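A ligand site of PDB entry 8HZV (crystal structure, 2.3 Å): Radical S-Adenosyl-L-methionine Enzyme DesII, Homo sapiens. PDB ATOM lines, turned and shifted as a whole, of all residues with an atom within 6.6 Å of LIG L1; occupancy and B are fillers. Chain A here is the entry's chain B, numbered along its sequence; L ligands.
The side-chain amide nitrogen (ND2) of Asn 216 lies close to a sulfur (S2) of LG2 L2 (3.3 Å). An iron atom (FE4) of LG2 L2 is bound by the side-chain sulfur of Cys 141. SG of Cys 145 binds FE3 of LG2 L2 (2.7 Å). A nitrogen (N1) of LIG L1 is in hydrogen-bond range of the backbone carbonyl oxygen (O) of Leu 189, 3.5 Å away. An iron atom (FE2) of LG2 L2 is bound by the side-chain sulfur (SG) of Cys 148 (2.6 Å). An oxygen (O1) of LIG L1 lies close to the side-chain hydroxyl (OH) of Tyr 242 (2.8 Å). OH of Tyr 242 sits close to S4 of LG2 L2 (3.4 Å). S1 of LG2 L2 lies close to N of Cys 145. The side-chain hydroxyl of Ser 240 lies within hydrogen-bond range of an oxygen (O2) of LIG L1 (2.5 Å). N1 of LIG L1 is in salt-bridge range of OE1 of Glu 190 (3.95 Å).
FE1 of LG2 L2 is bound by O1 of LIG L1 (2.6 Å).
The backbone carbonyl oxygen (O) of Arg 238 is in hydrogen-bond range of the backbone NH (N) of Thr 215, at 3.2 Å. N of Ser 217 lies within hydrogen-bond range of OG1 of Thr 215 (2.9 Å). The side-chain amide nitrogen of Asn 216 lies close to the side-chain sulfur of Cys 141, 3.7 Å away. The side-chain hydroxyl (OG1) of Thr 215 is in hydrogen-bond range of the side-chain carboxylate (OE2) of Glu 190. N of Asn 216 lies within hydrogen-bond range of OE1 of Glu 190 (2.8 Å). N of Ser 240 is in hydrogen-bond range of O of Thr 215, 2.8 Å away.
A sulfur (S1) of LIG L1 sits close to the backbone carbonyl oxygen (O) of Gly 187 (3.8 Å). A sulfur (S1) of LIG L1 sits close to the backbone carbonyl oxygen of Gly 188 (3.3 Å). Merely in contact with LIG L1: Glu 408 (3.2 Å), Thr 215 (3.5 Å), Phe 411 (3.7 Å) and Asn 216 (3.8 Å). Hydrophobic or aromatic side chains that line LIG L1: Tyr 242 and Phe 411.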
ATOM      1  N   TYR A 136      -5.178 -16.298  -7.709  1.00  0.00           N
ATOM      2  CA  TYR A 136      -5.323 -17.388  -6.751  1.00  0.00           C
ATOM      3  C   TYR A 136      -5.925 -16.818  -5.472  1.00  0.00           C
ATOM      4  O   TYR A 136      -5.188 -16.421  -4.557  1.00  0.00           O
ATOM      5  CB  TYR A 136      -3.971 -18.049  -6.465  1.00  0.00           C
ATOM      6  CG  TYR A 136      -3.364 -18.855  -7.610  1.00  0.00           C
ATOM      7  CD1 TYR A 136      -3.917 -18.822  -8.891  1.00  0.00           C
ATOM      8  CD2 TYR A 136      -2.244 -19.645  -7.405  1.00  0.00           C
ATOM      9  CE1 TYR A 136      -3.372 -19.563  -9.924  1.00  0.00           C
ATOM     10  CE2 TYR A 136      -1.685 -20.395  -8.434  1.00  0.00           C
ATOM     11  CZ  TYR A 136      -2.249 -20.354  -9.685  1.00  0.00           C
ATOM     12  OH  TYR A 136      -1.670 -21.098 -10.669  1.00  0.00           O
ATOM     13  N   CYS A 141      -8.300 -24.703   1.448  1.00  0.00           N
ATOM     14  CA  CYS A 141      -8.963 -25.787   0.749  1.00  0.00           C
ATOM     15  C   CYS A 141      -9.421 -26.833   1.754  1.00  0.00           C
ATOM     16  O   CYS A 141      -8.730 -27.093   2.754  1.00  0.00           O
ATOM     17  CB  CYS A 141      -8.085 -26.438  -0.295  1.00  0.00           C
ATOM     18  SG  CYS A 141      -9.066 -27.586  -1.245  1.00  0.00           S
ATOM     19  N   PHE A 143     -10.069 -29.999   0.704  1.00  0.00           N
ATOM     20  CA  PHE A 143      -9.530 -31.261   0.219  1.00  0.00           C
ATOM     21  C   PHE A 143      -8.050 -31.364   0.578  1.00  0.00           C
ATOM     22  O   PHE A 143      -7.424 -30.396   1.017  1.00  0.00           O
ATOM     23  CB  PHE A 143      -9.714 -31.381  -1.303  1.00  0.00           C
ATOM     24  CG  PHE A 143     -11.142 -31.625  -1.727  1.00  0.00           C
ATOM     25  CD1 PHE A 143     -12.170 -31.674  -0.803  1.00  0.00           C
ATOM     26  CD2 PHE A 143     -11.446 -31.816  -3.069  1.00  0.00           C
ATOM     27  CE1 PHE A 143     -13.473 -31.908  -1.212  1.00  0.00           C
ATOM     28  CE2 PHE A 143     -12.742 -32.037  -3.478  1.00  0.00           C
ATOM     29  CZ  PHE A 143     -13.762 -32.083  -2.549  1.00  0.00           C
ATOM     30  N   CYS A 145      -5.770 -33.526  -1.689  1.00  0.00           N
ATOM     31  CA  CYS A 145      -5.524 -34.452  -2.780  1.00  0.00           C
ATOM     32  C   CYS A 145      -4.086 -34.961  -2.732  1.00  0.00           C
ATOM     33  O   CYS A 145      -3.145 -34.195  -2.534  1.00  0.00           O
ATOM     34  CB  CYS A 145      -5.807 -33.768  -4.118  1.00  0.00           C
ATOM     35  SG  CYS A 145      -7.559 -33.445  -4.437  1.00  0.00           S
ATOM     36  N   PHE A 147      -2.093 -35.952  -4.950  1.00  0.00           N
ATOM     37  CA  PHE A 147      -1.215 -35.448  -5.988  1.00  0.00           C
ATOM     38  C   PHE A 147      -0.890 -33.967  -5.843  1.00  0.00           C
ATOM     39  O   PHE A 147       0.035 -33.484  -6.503  1.00  0.00           O
ATOM     40  CB  PHE A 147      -1.835 -35.692  -7.372  1.00  0.00           C
ATOM     41  CG  PHE A 147      -3.208 -35.088  -7.547  1.00  0.00           C
ATOM     42  CD1 PHE A 147      -3.353 -33.751  -7.876  1.00  0.00           C
ATOM     43  CD2 PHE A 147      -4.338 -35.861  -7.381  1.00  0.00           C
ATOM     44  CE1 PHE A 147      -4.612 -33.197  -8.018  1.00  0.00           C
ATOM     45  CE2 PHE A 147      -5.599 -35.315  -7.535  1.00  0.00           C
ATOM     46  CZ  PHE A 147      -5.728 -33.979  -7.848  1.00  0.00           C
ATOM     47  N   CYS A 148      -1.630 -33.234  -5.015  1.00  0.00           N
ATOM     48  CA  CYS A 148      -1.458 -31.799  -4.935  1.00  0.00           C
ATOM     49  C   CYS A 148      -0.271 -31.443  -4.047  1.00  0.00           C
ATOM     50  O   CYS A 148       0.018 -32.116  -3.046  1.00  0.00           O
ATOM     51  CB  CYS A 148      -2.727 -31.125  -4.406  1.00  0.00           C
ATOM     52  SG  CYS A 148      -2.524 -29.347  -4.073  1.00  0.00           S
ATOM     53  N   VAL A 149       0.430 -30.366  -4.421  1.00  0.00           N
ATOM     54  CA  VAL A 149       1.632 -29.944  -3.701  1.00  0.00           C
ATOM     55  C   VAL A 149       1.329 -29.101  -2.484  1.00  0.00           C
ATOM     56  O   VAL A 149       2.265 -28.704  -1.765  1.00  0.00           O
ATOM     57  CB  VAL A 149       2.591 -29.173  -4.633  1.00  0.00           C
ATOM     58  CG1 VAL A 149       3.070 -30.080  -5.766  1.00  0.00           C
ATOM     59  CG2 VAL A 149       1.916 -27.925  -5.179  1.00  0.00           C
ATOM     60  N   SER A 186      -8.112 -19.328 -10.558  1.00  0.00           N
ATOM     61  CA  SER A 186      -7.789 -20.700 -10.209  1.00  0.00           C
ATOM     62  C   SER A 186      -7.131 -20.687  -8.845  1.00  0.00           C
ATOM     63  O   SER A 186      -7.511 -19.887  -7.975  1.00  0.00           O
ATOM     64  CB  SER A 186      -6.866 -21.346 -11.246  1.00  0.00           C
ATOM     65  OG  SER A 186      -6.782 -22.742 -11.039  1.00  0.00           O
ATOM     66  N   GLY A 187      -6.142 -21.533  -8.633  1.00  0.00           N
ATOM     67  CA  GLY A 187      -5.446 -21.424  -7.377  1.00  0.00           C
ATOM     68  C   GLY A 187      -4.316 -22.407  -7.276  1.00  0.00           C
ATOM     69  O   GLY A 187      -4.137 -23.290  -8.109  1.00  0.00           O
ATOM     70  N   GLY A 188      -3.507 -22.156  -6.255  1.00  0.00           N
ATOM     71  CA  GLY A 188      -3.023 -23.217  -5.435  1.00  0.00           C
ATOM     72  C   GLY A 188      -4.233 -23.770  -4.716  1.00  0.00           C
ATOM     73  O   GLY A 188      -4.699 -24.849  -5.052  1.00  0.00           O
ATOM     74  N   LEU A 189      -4.787 -23.019  -3.775  1.00  0.00           N
ATOM     75  CA  LEU A 189      -5.894 -23.499  -2.949  1.00  0.00           C
ATOM     76  C   LEU A 189      -7.242 -23.292  -3.669  1.00  0.00           C
ATOM     77  O   LEU A 189      -7.302 -22.921  -4.846  1.00  0.00           O
ATOM     78  CB  LEU A 189      -5.865 -22.813  -1.591  1.00  0.00           C
ATOM     79  CG  LEU A 189      -4.553 -22.958  -0.796  1.00  0.00           C
ATOM     80  CD1 LEU A 189      -4.595 -22.135   0.480  1.00  0.00           C
ATOM     81  CD2 LEU A 189      -4.255 -24.408  -0.491  1.00  0.00           C
ATOM     82  N   GLU A 190      -8.336 -23.538  -2.945  1.00  0.00           N
ATOM     83  CA  GLU A 190      -9.679 -23.582  -3.520  1.00  0.00           C
ATOM     84  C   GLU A 190     -10.251 -22.167  -3.627  1.00  0.00           C
ATOM     85  O   GLU A 190     -10.395 -21.492  -2.604  1.00  0.00           O
ATOM     86  CB  GLU A 190     -10.575 -24.459  -2.656  1.00  0.00           C
ATOM     87  CG  GLU A 190     -12.027 -24.689  -3.112  1.00  0.00           C
ATOM     88  CD  GLU A 190     -12.248 -24.585  -4.608  1.00  0.00           C
ATOM     89  OE1 GLU A 190     -11.671 -25.409  -5.355  1.00  0.00           O
ATOM     90  OE2 GLU A 190     -13.015 -23.704  -5.035  1.00  0.00           O
ATOM     91  N   PRO A 191     -10.577 -21.686  -4.836  1.00  0.00           N
ATOM     92  CA  PRO A 191     -11.032 -20.291  -4.973  1.00  0.00           C
ATOM     93  C   PRO A 191     -12.336 -19.977  -4.261  1.00  0.00           C
ATOM     94  O   PRO A 191     -12.505 -18.844  -3.773  1.00  0.00           O
ATOM     95  CB  PRO A 191     -11.188 -20.122  -6.498  1.00  0.00           C
ATOM     96  CG  PRO A 191     -10.340 -21.181  -7.094  1.00  0.00           C
ATOM     97  CD  PRO A 191     -10.377 -22.336  -6.143  1.00  0.00           C
ATOM     98  N   TYR A 214     -11.579 -22.180 -12.027  1.00  0.00           N
ATOM     99  CA  TYR A 214     -11.218 -23.588 -11.891  1.00  0.00           C
ATOM    100  C   TYR A 214     -11.332 -23.953 -10.422  1.00  0.00           C
ATOM    101  O   TYR A 214     -10.620 -23.382  -9.588  1.00  0.00           O
ATOM    102  CB  TYR A 214      -9.806 -23.847 -12.434  1.00  0.00           C
ATOM    103  CG  TYR A 214      -9.672 -23.503 -13.899  1.00  0.00           C
ATOM    104  CD1 TYR A 214      -9.366 -22.211 -14.313  1.00  0.00           C
ATOM    105  CD2 TYR A 214      -9.858 -24.473 -14.875  1.00  0.00           C
ATOM    106  CE1 TYR A 214      -9.248 -21.893 -15.656  1.00  0.00           C
ATOM    107  CE2 TYR A 214      -9.742 -24.171 -16.223  1.00  0.00           C
ATOM    108  CZ  TYR A 214      -9.446 -22.878 -16.601  1.00  0.00           C
ATOM    109  OH  TYR A 214      -9.329 -22.560 -17.943  1.00  0.00           O
ATOM    110  N   THR A 215     -12.222 -24.890 -10.106  1.00  0.00           N
ATOM    111  CA  THR A 215     -12.588 -25.165  -8.718  1.00  0.00           C
ATOM    112  C   THR A 215     -12.907 -26.642  -8.556  1.00  0.00           C
ATOM    113  O   THR A 215     -13.175 -27.359  -9.535  1.00  0.00           O
ATOM    114  CB  THR A 215     -13.807 -24.334  -8.296  1.00  0.00           C
ATOM    115  OG1 THR A 215     -14.192 -24.686  -6.965  1.00  0.00           O
ATOM    116  CG2 THR A 215     -14.979 -24.583  -9.242  1.00  0.00           C
ATOM    117  N   ASN A 216     -12.867 -27.106  -7.304  1.00  0.00           N
ATOM    118  CA  ASN A 216     -13.374 -28.448  -6.997  1.00  0.00           C
ATOM    119  C   ASN A 216     -14.883 -28.448  -6.780  1.00  0.00           C
ATOM    120  O   ASN A 216     -15.459 -29.537  -6.617  1.00  0.00           O
ATOM    121  CB  ASN A 216     -12.660 -29.044  -5.762  1.00  0.00           C
ATOM    122  CG  ASN A 216     -12.873 -28.241  -4.479  1.00  0.00           C
ATOM    123  OD1 ASN A 216     -13.955 -27.717  -4.223  1.00  0.00           O
ATOM    124  ND2 ASN A 216     -11.836 -28.173  -3.656  1.00  0.00           N
ATOM    125  N   SER A 217     -15.508 -27.280  -6.752  1.00  0.00           N
ATOM    126  CA  SER A 217     -16.958 -27.090  -6.701  1.00  0.00           C
ATOM    127  C   SER A 217     -17.590 -27.688  -5.447  1.00  0.00           C
ATOM    128  O   SER A 217     -18.827 -27.753  -5.360  1.00  0.00           O
ATOM    129  CB  SER A 217     -17.636 -27.663  -7.945  1.00  0.00           C
ATOM    130  OG  SER A 217     -17.335 -26.894  -9.089  1.00  0.00           O
ATOM    131  N   ARG A 238     -15.091 -24.609 -14.632  1.00  0.00           N
ATOM    132  CA  ARG A 238     -14.568 -25.951 -14.879  1.00  0.00           C
ATOM    133  C   ARG A 238     -14.347 -26.626 -13.528  1.00  0.00           C
ATOM    134  O   ARG A 238     -13.499 -26.191 -12.735  1.00  0.00           O
ATOM    135  CB  ARG A 238     -13.280 -25.927 -15.698  1.00  0.00           C
ATOM    136  CG  ARG A 238     -13.003 -27.278 -16.366  1.00  0.00           C
ATOM    137  CD  ARG A 238     -11.602 -27.385 -16.916  1.00  0.00           C
ATOM    138  NE  ARG A 238     -10.596 -27.419 -15.853  1.00  0.00           N
ATOM    139  CZ  ARG A 238      -9.307 -27.619 -16.061  1.00  0.00           C
ATOM    140  NH1 ARG A 238      -8.850 -27.807 -17.294  1.00  0.00           N
ATOM    141  NH2 ARG A 238      -8.466 -27.629 -15.032  1.00  0.00           N
ATOM    142  N   THR A 239     -15.103 -27.691 -13.276  1.00  0.00           N
ATOM    143  CA  THR A 239     -14.985 -28.431 -12.037  1.00  0.00           C
ATOM    144  C   THR A 239     -13.950 -29.534 -12.201  1.00  0.00           C
ATOM    145  O   THR A 239     -14.019 -30.316 -13.150  1.00  0.00           O
ATOM    146  CB  THR A 239     -16.334 -29.035 -11.641  1.00  0.00           C
ATOM    147  OG1 THR A 239     -17.247 -27.988 -11.311  1.00  0.00           O
ATOM    148  CG2 THR A 239     -16.170 -29.970 -10.440  1.00  0.00           C
ATOM    149  N   SER A 240     -12.982 -29.584 -11.285  1.00  0.00           N
ATOM    150  CA  SER A 240     -12.037 -30.691 -11.225  1.00  0.00           C
ATOM    151  C   SER A 240     -12.746 -31.906 -10.643  1.00  0.00           C
ATOM    152  O   SER A 240     -12.995 -31.964  -9.432  1.00  0.00           O
ATOM    153  CB  SER A 240     -10.819 -30.317 -10.397  1.00  0.00           C
ATOM    154  OG  SER A 240     -10.076 -29.272 -11.015  1.00  0.00           O
ATOM    155  N   TYR A 242     -12.792 -35.459  -9.408  1.00  0.00           N
ATOM    156  CA  TYR A 242     -11.792 -36.372  -8.850  1.00  0.00           C
ATOM    157  C   TYR A 242     -12.317 -37.792  -8.659  1.00  0.00           C
ATOM    158  O   TYR A 242     -11.780 -38.530  -7.826  1.00  0.00           O
ATOM    159  CB  TYR A 242     -11.275 -35.804  -7.524  1.00  0.00           C
ATOM    160  CG  TYR A 242     -10.548 -34.501  -7.676  1.00  0.00           C
ATOM    161  CD1 TYR A 242      -9.573 -34.341  -8.650  1.00  0.00           C
ATOM    162  CD2 TYR A 242     -10.833 -33.417  -6.851  1.00  0.00           C
ATOM    163  CE1 TYR A 242      -8.897 -33.149  -8.805  1.00  0.00           C
ATOM    164  CE2 TYR A 242     -10.163 -32.221  -6.998  1.00  0.00           C
ATOM    165  CZ  TYR A 242      -9.190 -32.094  -7.967  1.00  0.00           C
ATOM    166  OH  TYR A 242      -8.508 -30.906  -8.128  1.00  0.00           O
ATOM    167  N   ARG A 407       2.988 -21.983 -12.013  1.00  0.00           N
ATOM    168  CA  ARG A 407       1.626 -22.189 -11.550  1.00  0.00           C
ATOM    169  C   ARG A 407       1.574 -22.955 -10.223  1.00  0.00           C
ATOM    170  O   ARG A 407       0.743 -22.645  -9.360  1.00  0.00           O
ATOM    171  CB  ARG A 407       0.813 -22.918 -12.614  1.00  0.00           C
ATOM    172  CG  ARG A 407       0.050 -21.999 -13.552  1.00  0.00           C
ATOM    173  CD  ARG A 407       0.858 -21.655 -14.789  1.00  0.00           C
ATOM    174  NE  ARG A 407       0.116 -20.738 -15.660  1.00  0.00           N
ATOM    175  CZ  ARG A 407      -0.750 -21.133 -16.590  1.00  0.00           C
ATOM    176  NH1 ARG A 407      -0.994 -22.422 -16.775  1.00  0.00           N
ATOM    177  NH2 ARG A 407      -1.387 -20.229 -17.339  1.00  0.00           N
ATOM    178  N   GLU A 408       2.424 -23.958 -10.063  1.00  0.00           N
ATOM    179  CA  GLU A 408       2.387 -24.800  -8.868  1.00  0.00           C
ATOM    180  C   GLU A 408       3.310 -24.305  -7.756  1.00  0.00           C
ATOM    181  O   GLU A 408       3.515 -25.024  -6.770  1.00  0.00           O
ATOM    182  CB  GLU A 408       2.754 -26.248  -9.233  1.00  0.00           C
ATOM    183  CG  GLU A 408       1.977 -26.819 -10.403  1.00  0.00           C
ATOM    184  CD  GLU A 408       0.500 -26.999 -10.094  1.00  0.00           C
ATOM    185  OE1 GLU A 408      -0.303 -27.071 -11.048  1.00  0.00           O
ATOM    186  OE2 GLU A 408       0.155 -27.069  -8.902  1.00  0.00           O
ATOM    187  N   PHE A 411       1.605 -21.679  -3.428  1.00  0.00           N
ATOM    188  CA  PHE A 411       0.997 -22.343  -2.289  1.00  0.00           C
ATOM    189  C   PHE A 411       1.673 -21.860  -1.017  1.00  0.00           C
ATOM    190  O   PHE A 411       2.906 -21.744  -0.974  1.00  0.00           O
ATOM    191  CB  PHE A 411       1.149 -23.869  -2.359  1.00  0.00           C
ATOM    192  CG  PHE A 411       0.365 -24.517  -3.466  1.00  0.00           C
ATOM    193  CD1 PHE A 411       0.815 -24.490  -4.775  1.00  0.00           C
ATOM    194  CD2 PHE A 411      -0.816 -25.198  -3.182  1.00  0.00           C
ATOM    195  CE1 PHE A 411       0.095 -25.100  -5.789  1.00  0.00           C
ATOM    196  CE2 PHE A 411      -1.528 -25.821  -4.180  1.00  0.00           C
ATOM    197  CZ  PHE A 411      -1.071 -25.782  -5.490  1.00  0.00           C
HETATM  198  N1  LIG L   1      -7.992 -25.762  -6.751  1.00  0.00           N
HETATM  199  C1  LIG L   1      -7.946 -26.326  -8.092  1.00  0.00           C
HETATM  200  C2  LIG L   1      -8.959 -27.444  -8.253  1.00  0.00           C
HETATM  201  O1  LIG L   1      -9.130 -28.281  -7.369  1.00  0.00           O
HETATM  202  C3  LIG L   1      -6.550 -26.844  -8.411  1.00  0.00           C
HETATM  203  C4  LIG L   1      -5.453 -26.071  -7.708  1.00  0.00           C
HETATM  204  S1  LIG L   1      -3.922 -26.983  -7.451  1.00  0.00           S
HETATM  205  C5  LIG L   1      -3.059 -26.623  -8.985  1.00  0.00           C
HETATM  206  O2  LIG L   1      -9.623 -27.554  -9.281  1.00  0.00           O
HETATM  207 FE1  LG2 L   2      -7.259 -28.324  -5.575  1.00  0.00          FE
HETATM  208 FE2  LG2 L   2      -5.106 -29.235  -4.149  1.00  0.00          FE
HETATM  209 FE3  LG2 L   2      -7.136 -30.812  -4.361  1.00  0.00          FE
HETATM  210 FE4  LG2 L   2      -7.355 -28.583  -2.851  1.00  0.00          FE
HETATM  211  S1  LG2 L   2      -5.987 -30.365  -2.397  1.00  0.00           S
HETATM  212  S2  LG2 L   2      -8.878 -29.343  -4.385  1.00  0.00           S
HETATM  213  S3  LG2 L   2      -6.070 -27.171  -3.980  1.00  0.00           S
HETATM  214  S4  LG2 L   2      -5.920 -30.113  -6.088  1.00  0.00           S
